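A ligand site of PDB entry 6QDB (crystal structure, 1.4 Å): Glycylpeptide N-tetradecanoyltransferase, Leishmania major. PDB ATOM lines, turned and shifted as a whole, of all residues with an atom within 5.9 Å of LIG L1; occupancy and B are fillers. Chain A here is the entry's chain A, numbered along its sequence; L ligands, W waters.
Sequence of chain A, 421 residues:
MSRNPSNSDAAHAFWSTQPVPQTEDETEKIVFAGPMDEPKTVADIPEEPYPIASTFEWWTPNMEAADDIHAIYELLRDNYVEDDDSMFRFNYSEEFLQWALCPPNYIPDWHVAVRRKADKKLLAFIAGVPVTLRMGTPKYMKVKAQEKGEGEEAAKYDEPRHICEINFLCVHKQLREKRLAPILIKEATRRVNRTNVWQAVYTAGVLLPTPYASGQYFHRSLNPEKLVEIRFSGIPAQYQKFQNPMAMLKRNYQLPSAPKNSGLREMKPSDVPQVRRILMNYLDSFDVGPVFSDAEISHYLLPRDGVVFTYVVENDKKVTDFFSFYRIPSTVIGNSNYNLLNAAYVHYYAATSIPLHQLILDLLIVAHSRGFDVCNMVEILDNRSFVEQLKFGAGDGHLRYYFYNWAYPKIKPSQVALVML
A nitrogen (N1) of LIG L1 is in hydrogen-bond range of the backbone NH of Gly 205, 3.4 Å away. A nitrogen (N3) of LIG L1 lies within hydrogen-bond range of the side-chain hydroxyl (OH) of Tyr 345 (2.7 Å). ND2 of Asn 376 is in hydrogen-bond range of N1 of LG2 L2, 3.1 Å away. O of Leu 421 is in salt-bridge range of N6 of LIG L1. The side-chain carboxylate (OD1) of Asp 396 is in salt-bridge range of a nitrogen (N6) of LG2 L2 (3.4 Å). OH of Tyr 217 is in hydrogen-bond range of N2 of LIG L1.
OH of Tyr 92 is in hydrogen-bond range of OXT of Leu 421 (2.6 Å). The backbone NH (N) of Phe 90 lies within hydrogen-bond range of the backbone carbonyl oxygen (O) of Val 81, 3.1 Å away. The side-chain hydroxyl of Tyr 345 sits close to the side-chain amide nitrogen of Asn 376. The side-chain amide oxygen (OD1) of Asn 167 sits at hydrogen-bond distance from the side-chain hydroxyl (OH) of Tyr 80 (3.4 Å). The backbone carbonyl oxygen of Gly 397 lies within hydrogen-bond range of the backbone NH of Tyr 217, 3.0 Å away. The chain-end carboxylate (O) of Leu 421 sits at hydrogen-bond distance from the side-chain amide nitrogen (ND2) of Asn 167, 2.8 Å away. The side-chain amide oxygen (OD1) of Asn 376 lies within hydrogen-bond range of a ring nitrogen (ND1) of His 219.
Phe 90 touches LIG L1 (CZ to C5, 3.3 Å). Tyr 92 touches LIG L1. Asn 167 touches LIG L1 (OD1 to N6, 3.8 Å). OG1 of Thr 203 touches C15 of LIG L1, at 3.7 Å. His 219 touches LIG L1. Ile 328 touches LIG L1. ND2 of Asn 376 touches C7 of LIG L1, at 3.9 Å. Gly 397 touches LIG L1. His 398 touches LIG L1 (O to C1, 3.7 Å). Met 420 touches LIG L1 (O to C16, 3.8 Å). Hydrophobic or aromatic side chains within 4 Å of LIG L1: Phe 90, Tyr 217, His 219, Ile 328 and Tyr 345. Of the 21 residues printed, 14 come within 4 Å of LIG L1. The nearest printed residue that does not touch LIG L1 is Ala 204 (4.04 Å).
Water W4 lies within hydrogen-bond range of OH of Tyr 80 (2.7 Å), OD1 of Asn 167 (2.7 Å), OH of Tyr 92 (2.8 Å), N6 of LIG L1 (2.9 Å) and O of Leu 421 (3.2 Å). Water W2 lies within hydrogen-bond range of the backbone NH (N) of Gly 205 (2.9 Å), the backbone NH (N) of Val 206 (3.0 Å) and a nitrogen (N1) of LIG L1 (3.3 Å). Water W6 bridges O of Met 420 (2.7 Å) and OXT of Leu 421 (2.8 Å).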
ATOM      1  N   TYR A  80      25.866   0.045   9.925  1.00  0.00           N
ATOM      2  CA  TYR A  80      24.603  -0.664  10.194  1.00  0.00           C
ATOM      3  C   TYR A  80      23.417   0.003   9.495  1.00  0.00           C
ATOM      4  O   TYR A  80      23.594   0.794   8.553  1.00  0.00           O
ATOM      5  CB  TYR A  80      24.406  -0.858  11.705  1.00  0.00           C
ATOM      6  CG  TYR A  80      23.456  -2.008  12.084  1.00  0.00           C
ATOM      7  CD1 TYR A  80      23.535  -3.270  11.529  1.00  0.00           C
ATOM      8  CD2 TYR A  80      22.496  -1.800  13.075  1.00  0.00           C
ATOM      9  CE1 TYR A  80      22.706  -4.320  11.967  1.00  0.00           C
ATOM     10  CE2 TYR A  80      21.633  -2.827  13.510  1.00  0.00           C
ATOM     11  CZ  TYR A  80      21.727  -4.075  12.917  1.00  0.00           C
ATOM     12  OH  TYR A  80      20.875  -5.080  13.337  1.00  0.00           O
ATOM     13  N   VAL A  81      22.200  -0.390   9.851  1.00  0.00           N
ATOM     14  CA  VAL A  81      21.054  -0.052   8.989  1.00  0.00           C
ATOM     15  C   VAL A  81      20.842   1.475   8.879  1.00  0.00           C
ATOM     16  O   VAL A  81      20.891   2.203   9.869  1.00  0.00           O
ATOM     17  CB  VAL A  81      19.733  -0.689   9.495  1.00  0.00           C
ATOM     18  CG1 VAL A  81      18.689  -0.632   8.370  1.00  0.00           C
ATOM     19  CG2 VAL A  81      19.868  -2.134   9.980  1.00  0.00           C
ATOM     20  N   PHE A  90      21.443   3.815  12.415  1.00  0.00           N
ATOM     21  CA  PHE A  90      21.458   3.486  13.849  1.00  0.00           C
ATOM     22  C   PHE A  90      22.839   3.635  14.485  1.00  0.00           C
ATOM     23  O   PHE A  90      23.858   3.409  13.852  1.00  0.00           O
ATOM     24  CB  PHE A  90      21.050   2.026  14.065  1.00  0.00           C
ATOM     25  CG  PHE A  90      19.591   1.764  13.749  1.00  0.00           C
ATOM     26  CD1 PHE A  90      18.563   2.412  14.447  1.00  0.00           C
ATOM     27  CD2 PHE A  90      19.227   0.843  12.745  1.00  0.00           C
ATOM     28  CE1 PHE A  90      17.221   2.188  14.112  1.00  0.00           C
ATOM     29  CE2 PHE A  90      17.890   0.627  12.412  1.00  0.00           C
ATOM     30  CZ  PHE A  90      16.896   1.297  13.085  1.00  0.00           C
ATOM     31  N   TYR A  92      23.581   2.342  17.943  1.00  0.00           N
ATOM     32  CA  TYR A  92      23.460   1.600  19.189  1.00  0.00           C
ATOM     33  C   TYR A  92      24.685   1.869  20.085  1.00  0.00           C
ATOM     34  O   TYR A  92      25.823   1.791  19.608  1.00  0.00           O
ATOM     35  CB  TYR A  92      23.397   0.099  18.899  1.00  0.00           C
ATOM     36  CG  TYR A  92      22.099  -0.448  18.331  1.00  0.00           C
ATOM     37  CD1 TYR A  92      21.832  -0.441  16.971  1.00  0.00           C
ATOM     38  CD2 TYR A  92      21.127  -1.002  19.195  1.00  0.00           C
ATOM     39  CE1 TYR A  92      20.638  -0.956  16.474  1.00  0.00           C
ATOM     40  CE2 TYR A  92      19.964  -1.559  18.687  1.00  0.00           C
ATOM     41  CZ  TYR A  92      19.739  -1.579  17.321  1.00  0.00           C
ATOM     42  OH  TYR A  92      18.601  -2.189  16.809  1.00  0.00           O
ATOM     43  N   ASN A 167      20.890 -11.269  15.624  1.00  0.00           N
ATOM     44  CA  ASN A 167      20.757  -9.822  15.430  1.00  0.00           C
ATOM     45  C   ASN A 167      22.128  -9.249  15.032  1.00  0.00           C
ATOM     46  O   ASN A 167      23.150  -9.936  15.101  1.00  0.00           O
ATOM     47  CB  ASN A 167      20.251  -9.212  16.766  1.00  0.00           C
ATOM     48  CG  ASN A 167      19.466  -7.919  16.617  1.00  0.00           C
ATOM     49  OD1 ASN A 167      19.523  -7.195  15.634  1.00  0.00           O
ATOM     50  ND2 ASN A 167      18.505  -7.713  17.535  1.00  0.00           N
ATOM     51  N   THR A 203      14.619 -11.028  12.858  1.00  0.00           N
ATOM     52  CA  THR A 203      13.733 -10.062  12.181  1.00  0.00           C
ATOM     53  C   THR A 203      14.519  -9.283  11.139  1.00  0.00           C
ATOM     54  O   THR A 203      15.741  -9.194  11.186  1.00  0.00           O
ATOM     55  CB  THR A 203      13.054  -9.077  13.131  1.00  0.00           C
ATOM     56  OG1 THR A 203      14.060  -8.405  13.918  1.00  0.00           O
ATOM     57  CG2 THR A 203      12.074  -9.751  14.045  1.00  0.00           C
ATOM     58  N   ALA A 204      13.809  -8.731  10.143  1.00  0.00           N
ATOM     59  CA  ALA A 204      14.411  -7.731   9.242  1.00  0.00           C
ATOM     60  C   ALA A 204      13.307  -6.810   8.717  1.00  0.00           C
ATOM     61  O   ALA A 204      12.130  -7.155   8.766  1.00  0.00           O
ATOM     62  CB  ALA A 204      15.104  -8.430   8.081  1.00  0.00           C
ATOM     63  N   GLY A 205      13.724  -5.653   8.190  1.00  0.00           N
ATOM     64  CA  GLY A 205      12.833  -4.757   7.463  1.00  0.00           C
ATOM     65  C   GLY A 205      12.585  -5.295   6.057  1.00  0.00           C
ATOM     66  O   GLY A 205      11.447  -5.181   5.527  1.00  0.00           O
ATOM     67  N   VAL A 206      13.578  -5.906   5.442  1.00  0.00           N
ATOM     68  CA  VAL A 206      13.507  -6.403   4.080  1.00  0.00           C
ATOM     69  C   VAL A 206      12.698  -7.697   4.057  1.00  0.00           C
ATOM     70  O   VAL A 206      12.611  -8.450   5.042  1.00  0.00           O
ATOM     71  CB  VAL A 206      14.889  -6.563   3.438  1.00  0.00           C
ATOM     72  CG1 VAL A 206      15.541  -5.192   3.304  1.00  0.00           C
ATOM     73  CG2 VAL A 206      15.836  -7.522   4.168  1.00  0.00           C
ATOM     74  N   TYR A 217       5.692  -0.454  11.639  1.00  0.00           N
ATOM     75  CA  TYR A 217       6.169   0.473  12.657  1.00  0.00           C
ATOM     76  C   TYR A 217       5.198   1.637  12.885  1.00  0.00           C
ATOM     77  O   TYR A 217       4.541   2.125  11.945  1.00  0.00           O
ATOM     78  CB  TYR A 217       7.535   1.075  12.256  1.00  0.00           C
ATOM     79  CG  TYR A 217       8.719   0.240  12.722  1.00  0.00           C
ATOM     80  CD1 TYR A 217       9.191   0.350  14.012  1.00  0.00           C
ATOM     81  CD2 TYR A 217       9.272  -0.773  11.909  1.00  0.00           C
ATOM     82  CE1 TYR A 217      10.176  -0.508  14.512  1.00  0.00           C
ATOM     83  CE2 TYR A 217      10.287  -1.596  12.387  1.00  0.00           C
ATOM     84  CZ  TYR A 217      10.740  -1.462  13.684  1.00  0.00           C
ATOM     85  OH  TYR A 217      11.650  -2.377  14.166  1.00  0.00           O
ATOM     86  N   HIS A 219       5.064   5.504  15.237  1.00  0.00           N
ATOM     87  CA  HIS A 219       5.898   6.556  15.837  1.00  0.00           C
ATOM     88  C   HIS A 219       4.995   7.553  16.538  1.00  0.00           C
ATOM     89  O   HIS A 219       3.927   7.918  16.047  1.00  0.00           O
ATOM     90  CB  HIS A 219       6.724   7.258  14.752  1.00  0.00           C
ATOM     91  CG  HIS A 219       7.384   6.302  13.790  1.00  0.00           C
ATOM     92  ND1 HIS A 219       8.453   5.530  14.179  1.00  0.00           N
ATOM     93  CD2 HIS A 219       7.080   5.926  12.511  1.00  0.00           C
ATOM     94  CE1 HIS A 219       8.776   4.710  13.188  1.00  0.00           C
ATOM     95  NE2 HIS A 219       7.954   4.884  12.170  1.00  0.00           N
ATOM     96  N   PHE A 232      12.535  13.678   9.755  1.00  0.00           N
ATOM     97  CA  PHE A 232      12.012  12.394  10.195  1.00  0.00           C
ATOM     98  C   PHE A 232      10.518  12.420   9.865  1.00  0.00           C
ATOM     99  O   PHE A 232       9.984  11.440   9.434  1.00  0.00           O
ATOM    100  CB  PHE A 232      12.166  12.278  11.731  1.00  0.00           C
ATOM    101  CG  PHE A 232      11.607  11.034  12.378  1.00  0.00           C
ATOM    102  CD1 PHE A 232      10.247  10.864  12.598  1.00  0.00           C
ATOM    103  CD2 PHE A 232      12.454   9.988  12.689  1.00  0.00           C
ATOM    104  CE1 PHE A 232       9.777   9.699  13.195  1.00  0.00           C
ATOM    105  CE2 PHE A 232      11.981   8.831  13.309  1.00  0.00           C
ATOM    106  CZ  PHE A 232      10.631   8.709  13.553  1.00  0.00           C
ATOM    107  N   ILE A 328      17.564   3.680  21.530  1.00  0.00           N
ATOM    108  CA  ILE A 328      18.464   3.495  20.378  1.00  0.00           C
ATOM    109  C   ILE A 328      18.629   4.845  19.683  1.00  0.00           C
ATOM    110  O   ILE A 328      17.676   5.334  19.051  1.00  0.00           O
ATOM    111  CB  ILE A 328      17.954   2.439  19.366  1.00  0.00           C
ATOM    112  CG1 ILE A 328      17.587   1.123  20.078  1.00  0.00           C
ATOM    113  CG2 ILE A 328      19.083   2.272  18.304  1.00  0.00           C
ATOM    114  CD1 ILE A 328      16.931   0.130  19.102  1.00  0.00           C
ATOM    115  N   TYR A 345      11.995   3.133  22.506  1.00  0.00           N
ATOM    116  CA  TYR A 345      11.236   2.031  21.904  1.00  0.00           C
ATOM    117  C   TYR A 345      10.460   1.326  23.009  1.00  0.00           C
ATOM    118  O   TYR A 345      10.982   1.000  24.096  1.00  0.00           O
ATOM    119  CB  TYR A 345      12.208   0.978  21.322  1.00  0.00           C
ATOM    120  CG  TYR A 345      12.757   1.387  19.967  1.00  0.00           C
ATOM    121  CD1 TYR A 345      13.724   2.396  19.871  1.00  0.00           C
ATOM    122  CD2 TYR A 345      12.346   0.757  18.793  1.00  0.00           C
ATOM    123  CE1 TYR A 345      14.238   2.756  18.638  1.00  0.00           C
ATOM    124  CE2 TYR A 345      12.849   1.143  17.536  1.00  0.00           C
ATOM    125  CZ  TYR A 345      13.807   2.142  17.499  1.00  0.00           C
ATOM    126  OH  TYR A 345      14.347   2.491  16.242  1.00  0.00           O
ATOM    127  N   ASN A 376       8.986   4.806  19.410  1.00  0.00           N
ATOM    128  CA  ASN A 376       8.751   3.851  18.304  1.00  0.00           C
ATOM    129  C   ASN A 376       8.260   2.518  18.844  1.00  0.00           C
ATOM    130  O   ASN A 376       8.613   2.118  19.982  1.00  0.00           O
ATOM    131  CB  ASN A 376      10.087   3.585  17.580  1.00  0.00           C
ATOM    132  CG  ASN A 376      10.646   4.831  16.923  1.00  0.00           C
ATOM    133  OD1 ASN A 376       9.922   5.680  16.444  1.00  0.00           O
ATOM    134  ND2 ASN A 376      11.973   4.923  16.796  1.00  0.00           N
ATOM    135  N   ASP A 396       6.544   4.292   7.376  1.00  0.00           N
ATOM    136  CA  ASP A 396       6.755   3.578   6.102  1.00  0.00           C
ATOM    137  C   ASP A 396       7.390   2.194   6.276  1.00  0.00           C
ATOM    138  O   ASP A 396       7.433   1.393   5.319  1.00  0.00           O
ATOM    139  CB  ASP A 396       7.607   4.406   5.125  1.00  0.00           C
ATOM    140  CG  ASP A 396       8.974   4.847   5.644  1.00  0.00           C
ATOM    141  OD1 ASP A 396       9.279   4.731   6.860  1.00  0.00           O
ATOM    142  OD2 ASP A 396       9.768   5.344   4.793  1.00  0.00           O
ATOM    143  N   GLY A 397       7.830   1.913   7.489  1.00  0.00           N
ATOM    144  CA  GLY A 397       8.631   0.708   7.767  1.00  0.00           C
ATOM    145  C   GLY A 397       7.769  -0.447   8.259  1.00  0.00           C
ATOM    146  O   GLY A 397       6.673  -0.245   8.812  1.00  0.00           O
ATOM    147  N   HIS A 398       8.383  -1.640   8.154  1.00  0.00           N
ATOM    148  CA  HIS A 398       7.783  -2.835   8.731  1.00  0.00           C
ATOM    149  C   HIS A 398       8.870  -3.623   9.438  1.00  0.00           C
ATOM    150  O   HIS A 398      10.092  -3.438   9.190  1.00  0.00           O
ATOM    151  CB  HIS A 398       7.220  -3.744   7.635  1.00  0.00           C
ATOM    152  CG  HIS A 398       6.108  -3.126   6.840  1.00  0.00           C
ATOM    153  ND1 HIS A 398       6.295  -2.263   5.752  1.00  0.00           N
ATOM    154  CD2 HIS A 398       4.798  -3.311   6.993  1.00  0.00           C
ATOM    155  CE1 HIS A 398       5.094  -1.927   5.293  1.00  0.00           C
ATOM    156  NE2 HIS A 398       4.152  -2.550   6.024  1.00  0.00           N
ATOM    157  N   LEU A 399       8.468  -4.450  10.388  1.00  0.00           N
ATOM    158  CA  LEU A 399       9.343  -5.493  10.929  1.00  0.00           C
ATOM    159  C   LEU A 399       8.747  -6.848  10.611  1.00  0.00           C
ATOM    160  O   LEU A 399       7.607  -7.128  11.000  1.00  0.00           O
ATOM    161  CB  LEU A 399       9.618  -5.297  12.428  1.00  0.00           C
ATOM    162  CG  LEU A 399      10.865  -6.062  12.934  1.00  0.00           C
ATOM    163  CD1 LEU A 399      12.139  -5.546  12.312  1.00  0.00           C
ATOM    164  CD2 LEU A 399      10.986  -6.067  14.418  1.00  0.00           C
ATOM    165  N   MET A 420      12.066  -7.474  19.570  1.00  0.00           N
ATOM    166  CA  MET A 420      13.386  -7.673  18.999  1.00  0.00           C
ATOM    167  C   MET A 420      14.148  -6.345  18.969  1.00  0.00           C
ATOM    168  O   MET A 420      13.636  -5.326  18.477  1.00  0.00           O
ATOM    169  CB  MET A 420      13.261  -8.368  17.634  1.00  0.00           C
ATOM    170  CG  MET A 420      12.743  -9.839  17.804  1.00  0.00           C
ATOM    171  SD  MET A 420      13.982 -11.005  18.345  1.00  0.00           S
ATOM    172  CE  MET A 420      14.640 -11.620  16.792  1.00  0.00           C
ATOM    173  N   LEU A 421      15.348  -6.362  19.578  1.00  0.00           N
ATOM    174  CA  LEU A 421      16.121  -5.137  19.799  1.00  0.00           C
ATOM    175  C   LEU A 421      16.762  -4.600  18.511  1.00  0.00           C
ATOM    176  O   LEU A 421      17.090  -5.264  17.533  1.00  0.00           O
ATOM    177  CB  LEU A 421      17.240  -5.464  20.819  1.00  0.00           C
ATOM    178  CG  LEU A 421      16.724  -5.904  22.207  1.00  0.00           C
ATOM    179  CD1 LEU A 421      17.922  -6.151  23.106  1.00  0.00           C
ATOM    180  CD2 LEU A 421      15.783  -4.927  22.893  1.00  0.00           C
ATOM    181  OXT LEU A 421      16.900  -3.300  18.498  1.00  0.00           O
HETATM  182  C1  LIG L   1      13.438  -2.062  10.173  1.00  0.00           C
HETATM  183  C2  LIG L   1      14.935  -1.921   9.729  1.00  0.00           C
HETATM  184  C3  LIG L   1      15.702  -3.153   9.833  1.00  0.00           C
HETATM  185  C4  LIG L   1      13.162  -0.114  11.621  1.00  0.00           C
HETATM  186  C5  LIG L   1      14.109  -0.334  13.728  1.00  0.00           C
HETATM  187  C6  LIG L   1      12.985   1.638  13.264  1.00  0.00           C
HETATM  188  C7  LIG L   1      12.537   2.958  13.531  1.00  0.00           C
HETATM  189  N1  LIG L   1      16.239  -4.191   9.894  1.00  0.00           N
HETATM  190  N2  LIG L   1      13.892  -0.869  12.499  1.00  0.00           N
HETATM  191  N3  LIG L   1      13.723   0.869  14.170  1.00  0.00           N
HETATM  192  C8  LIG L   1      12.743   1.124  12.021  1.00  0.00           C
HETATM  193  C9  LIG L   1      11.886   3.368  12.278  1.00  0.00           C
HETATM  194  N4  LIG L   1      12.951  -0.764  10.433  1.00  0.00           N
HETATM  195  C10 LIG L   1      12.076  -0.069   9.413  1.00  0.00           C
HETATM  196  S1  LIG L   1      11.872   2.313  11.085  1.00  0.00           S
HETATM  197  N5  LIG L   1      14.855  -1.177  14.530  1.00  0.00           N
HETATM  198  C11 LIG L   1      15.399  -0.661  15.788  1.00  0.00           C
HETATM  199  C12 LIG L   1      15.130  -2.608  14.148  1.00  0.00           C
HETATM  200  C13 LIG L   1      16.599  -2.748  13.668  1.00  0.00           C
HETATM  201  C14 LIG L   1      16.883  -4.238  13.343  1.00  0.00           C
HETATM  202  N6  LIG L   1      16.556  -5.112  14.498  1.00  0.00           N
HETATM  203  C15 LIG L   1      15.163  -4.986  14.976  1.00  0.00           C
HETATM  204  C16 LIG L   1      14.837  -3.517  15.347  1.00  0.00           C
HETATM  205  C1  LG2 L   2      16.409   5.898  12.503  1.00  0.00           C
HETATM  206  C2  LG2 L   2      15.453   5.047  13.369  1.00  0.00           C
HETATM  207  C3  LG2 L   2      14.736   5.856  14.332  1.00  0.00           C
HETATM  208  C4  LG2 L   2      15.763   4.733  10.360  1.00  0.00           C
HETATM  209  C5  LG2 L   2      13.687   5.545   9.567  1.00  0.00           C
HETATM  210  C6  LG2 L   2      14.634   3.650   8.514  1.00  0.00           C
HETATM  211  C7  LG2 L   2      14.709   2.540   7.566  1.00  0.00           C
HETATM  212  N1  LG2 L   2      14.170   6.463  15.168  1.00  0.00           N
HETATM  213  N2  LG2 L   2      14.749   5.581  10.449  1.00  0.00           N
HETATM  214  N3  LG2 L   2      13.630   4.594   8.588  1.00  0.00           N
HETATM  215  C8  LG2 L   2      15.760   3.737   9.369  1.00  0.00           C
HETATM  216  C9  LG2 L   2      15.891   1.779   7.731  1.00  0.00           C
HETATM  217  N4  LG2 L   2      16.693   4.963  11.356  1.00  0.00           N
HETATM  218  C10 LG2 L   2      18.005   4.288  11.255  1.00  0.00           C
HETATM  219  S1  LG2 L   2      16.800   2.432   9.082  1.00  0.00           S
HETATM  220  N5  LG2 L   2      12.714   6.540   9.780  1.00  0.00           N
HETATM  221  C11 LG2 L   2      12.908   7.546  10.806  1.00  0.00           C
HETATM  222  C12 LG2 L   2      11.556   6.654   8.907  1.00  0.00           C
HETATM  223  C13 LG2 L   2      10.331   6.876   9.828  1.00  0.00           C
HETATM  224  C14 LG2 L   2       9.071   6.959   8.956  1.00  0.00           C
HETATM  225  N6  LG2 L   2       9.367   7.975   7.943  1.00  0.00           N
HETATM  226  C15 LG2 L   2      10.545   7.929   7.081  1.00  0.00           C
HETATM  227  C16 LG2 L   2      11.803   7.857   7.966  1.00  0.00           C
HETATM  228  S1  LG3 L   3      18.513  -7.572  10.126  1.00  0.00           S
HETATM  229  C1  LG3 L   3      19.742  -6.189   9.970  1.00  0.00           C
HETATM  230  C2  LG3 L   3      20.652  -6.473   8.749  1.00  0.00           C
HETATM  231  N1  LG3 L   3      21.738  -5.490   8.678  1.00  0.00           N
HETATM  232  C3  LG3 L   3      21.721  -4.424   7.893  1.00  0.00           C
HETATM  233  O1  LG3 L   3      20.720  -4.155   7.231  1.00  0.00           O
HETATM  234  C4  LG3 L   3      22.917  -3.536   7.984  1.00  0.00           C
HETATM  235  C5  LG3 L   3      23.281  -2.851   6.621  1.00  0.00           C
HETATM  236  N2  LG3 L   3      23.528  -3.845   5.550  1.00  0.00           N
HETATM  237  C6  LG3 L   3      24.500  -4.726   5.545  1.00  0.00           C
HETATM  238  O2  LG3 L   3      25.327  -4.748   6.450  1.00  0.00           O
HETATM  239  C7  LG3 L   3      24.529  -5.684   4.389  1.00  0.00           C
HETATM  240  O3  LG3 L   3      23.762  -5.146   3.316  1.00  0.00           O
HETATM  241  C8  LG3 L   3      24.005  -7.125   4.775  1.00  0.00           C
HETATM  242  C9  LG3 L   3      23.968  -8.031   3.591  1.00  0.00           C
HETATM  243  C10 LG3 L   3      22.578  -7.081   5.364  1.00  0.00           C
HETATM  244  C11 LG3 L   3      24.949  -7.774   5.819  1.00  0.00           C
HETATM  245  N3  LG3 L   3      19.046 -10.874   6.575  1.00  0.00           N
HETATM  246  O4  LG3 L   3      26.956 -10.404   1.316  1.00  0.00           O
HETATM  247  P1  LG3 L   3      25.921 -10.250   0.311  1.00  0.00           P
HETATM  248  C12 LG3 L   3      20.785 -11.761   1.814  1.00  0.00           C
HETATM  249  C13 LG3 L   3      19.309 -12.051   5.941  1.00  0.00           C
HETATM  250  O5  LG3 L   3      26.393 -10.227  -1.120  1.00  0.00           O
HETATM  251  P2  LG3 L   3      25.467  -7.582   1.395  1.00  0.00           P
HETATM  252  C14 LG3 L   3      19.442  -8.726  11.061  1.00  0.00           C
HETATM  253  O6  LG3 L   3      20.501  -8.394  11.651  1.00  0.00           O
HETATM  254  C15 LG3 L   3      20.312 -11.459   0.388  1.00  0.00           C
HETATM  255  O7  LG3 L   3      18.940 -11.744   0.254  1.00  0.00           O
HETATM  256  N4  LG3 L   3      19.749 -12.141   4.676  1.00  0.00           N
HETATM  257  O8  LG3 L   3      25.059  -8.880   0.556  1.00  0.00           O
HETATM  258  C16 LG3 L   3      18.930 -10.135  11.176  1.00  0.00           C
HETATM  259  C17 LG3 L   3      21.296 -12.367  -0.381  1.00  0.00           C
HETATM  260  O9  LG3 L   3      20.833 -13.717  -0.333  1.00  0.00           O
HETATM  261  P3  LG3 L   3      20.060 -14.297  -1.652  1.00  0.00           P
HETATM  262  C18 LG3 L   3      19.965 -10.953   4.041  1.00  0.00           C
HETATM  263  O10 LG3 L   3      24.465  -6.545   1.049  1.00  0.00           O
HETATM  264  C19 LG3 L   3      19.887 -11.025  10.318  1.00  0.00           C
HETATM  265  C20 LG3 L   3      22.609 -12.284   0.391  1.00  0.00           C
HETATM  266  O11 LG3 L   3      22.193 -11.753   1.706  1.00  0.00           O
HETATM  267  C21 LG3 L   3      19.696  -9.733   4.624  1.00  0.00           C
HETATM  268  O12 LG3 L   3      26.853  -7.241   1.255  1.00  0.00           O
HETATM  269  C22 LG3 L   3      19.384 -12.454  10.126  1.00  0.00           C
HETATM  270  C23 LG3 L   3      23.574 -11.249  -0.185  1.00  0.00           C
HETATM  271  O13 LG3 L   3      24.783 -11.322   0.554  1.00  0.00           O
HETATM  272  C24 LG3 L   3      19.212  -9.727   5.938  1.00  0.00           C
HETATM  273  N5  LG3 L   3      18.884  -8.568   6.618  1.00  0.00           N
HETATM  274  O14 LG3 L   3      25.307  -8.016   2.965  1.00  0.00           O
HETATM  275  C25 LG3 L   3      20.381 -13.313   9.328  1.00  0.00           C
HETATM  276  N6  LG3 L   3      20.030  -8.724   3.723  1.00  0.00           N
HETATM  277  O15 LG3 L   3      18.852 -13.397  -1.852  1.00  0.00           O
HETATM  278  C26 LG3 L   3      19.915 -14.774   9.118  1.00  0.00           C
HETATM  279  C27 LG3 L   3      20.428  -9.378   2.623  1.00  0.00           C
HETATM  280  O16 LG3 L   3      21.071 -14.155  -2.734  1.00  0.00           O
HETATM  281  C28 LG3 L   3      20.047 -15.626  10.367  1.00  0.00           C
HETATM  282  N7  LG3 L   3      20.419 -10.725   2.802  1.00  0.00           N
HETATM  283  O17 LG3 L   3      19.670 -15.662  -1.327  1.00  0.00           O
HETATM  284  C29 LG3 L   3      19.653 -17.067  10.090  1.00  0.00           C
HETATM  285  C30 LG3 L   3      19.793 -18.013  11.304  1.00  0.00           C
HETATM  286  C31 LG3 L   3      21.281 -18.360  11.597  1.00  0.00           C
HETATM  287  C32 LG3 L   3      21.461 -19.268  12.842  1.00  0.00           C
HETATM  288  C33 LG3 L   3      20.754 -20.615  12.764  1.00  0.00           C
HETATM  289  C34 LG3 L   3      21.005 -21.427  14.067  1.00  0.00           C
HETATM  290  C35 LG3 L   3      20.194 -22.742  14.039  1.00  0.00           C
HETATM  291  O   HOH W   1      17.079  -7.593  13.332  1.00  0.00           O
HETATM  292  O   HOH W   2      16.139  -4.953   6.685  1.00  0.00           O
HETATM  293  O   HOH W   3      10.958   3.366   8.015  1.00  0.00           O
HETATM  294  O   HOH W   4      19.241  -4.504  15.347  1.00  0.00           O
HETATM  295  O   HOH W   5      15.422  -2.128   6.440  1.00  0.00           O
HETATM  296  O   HOH W   6      14.145  -2.630  18.562  1.00  0.00           O
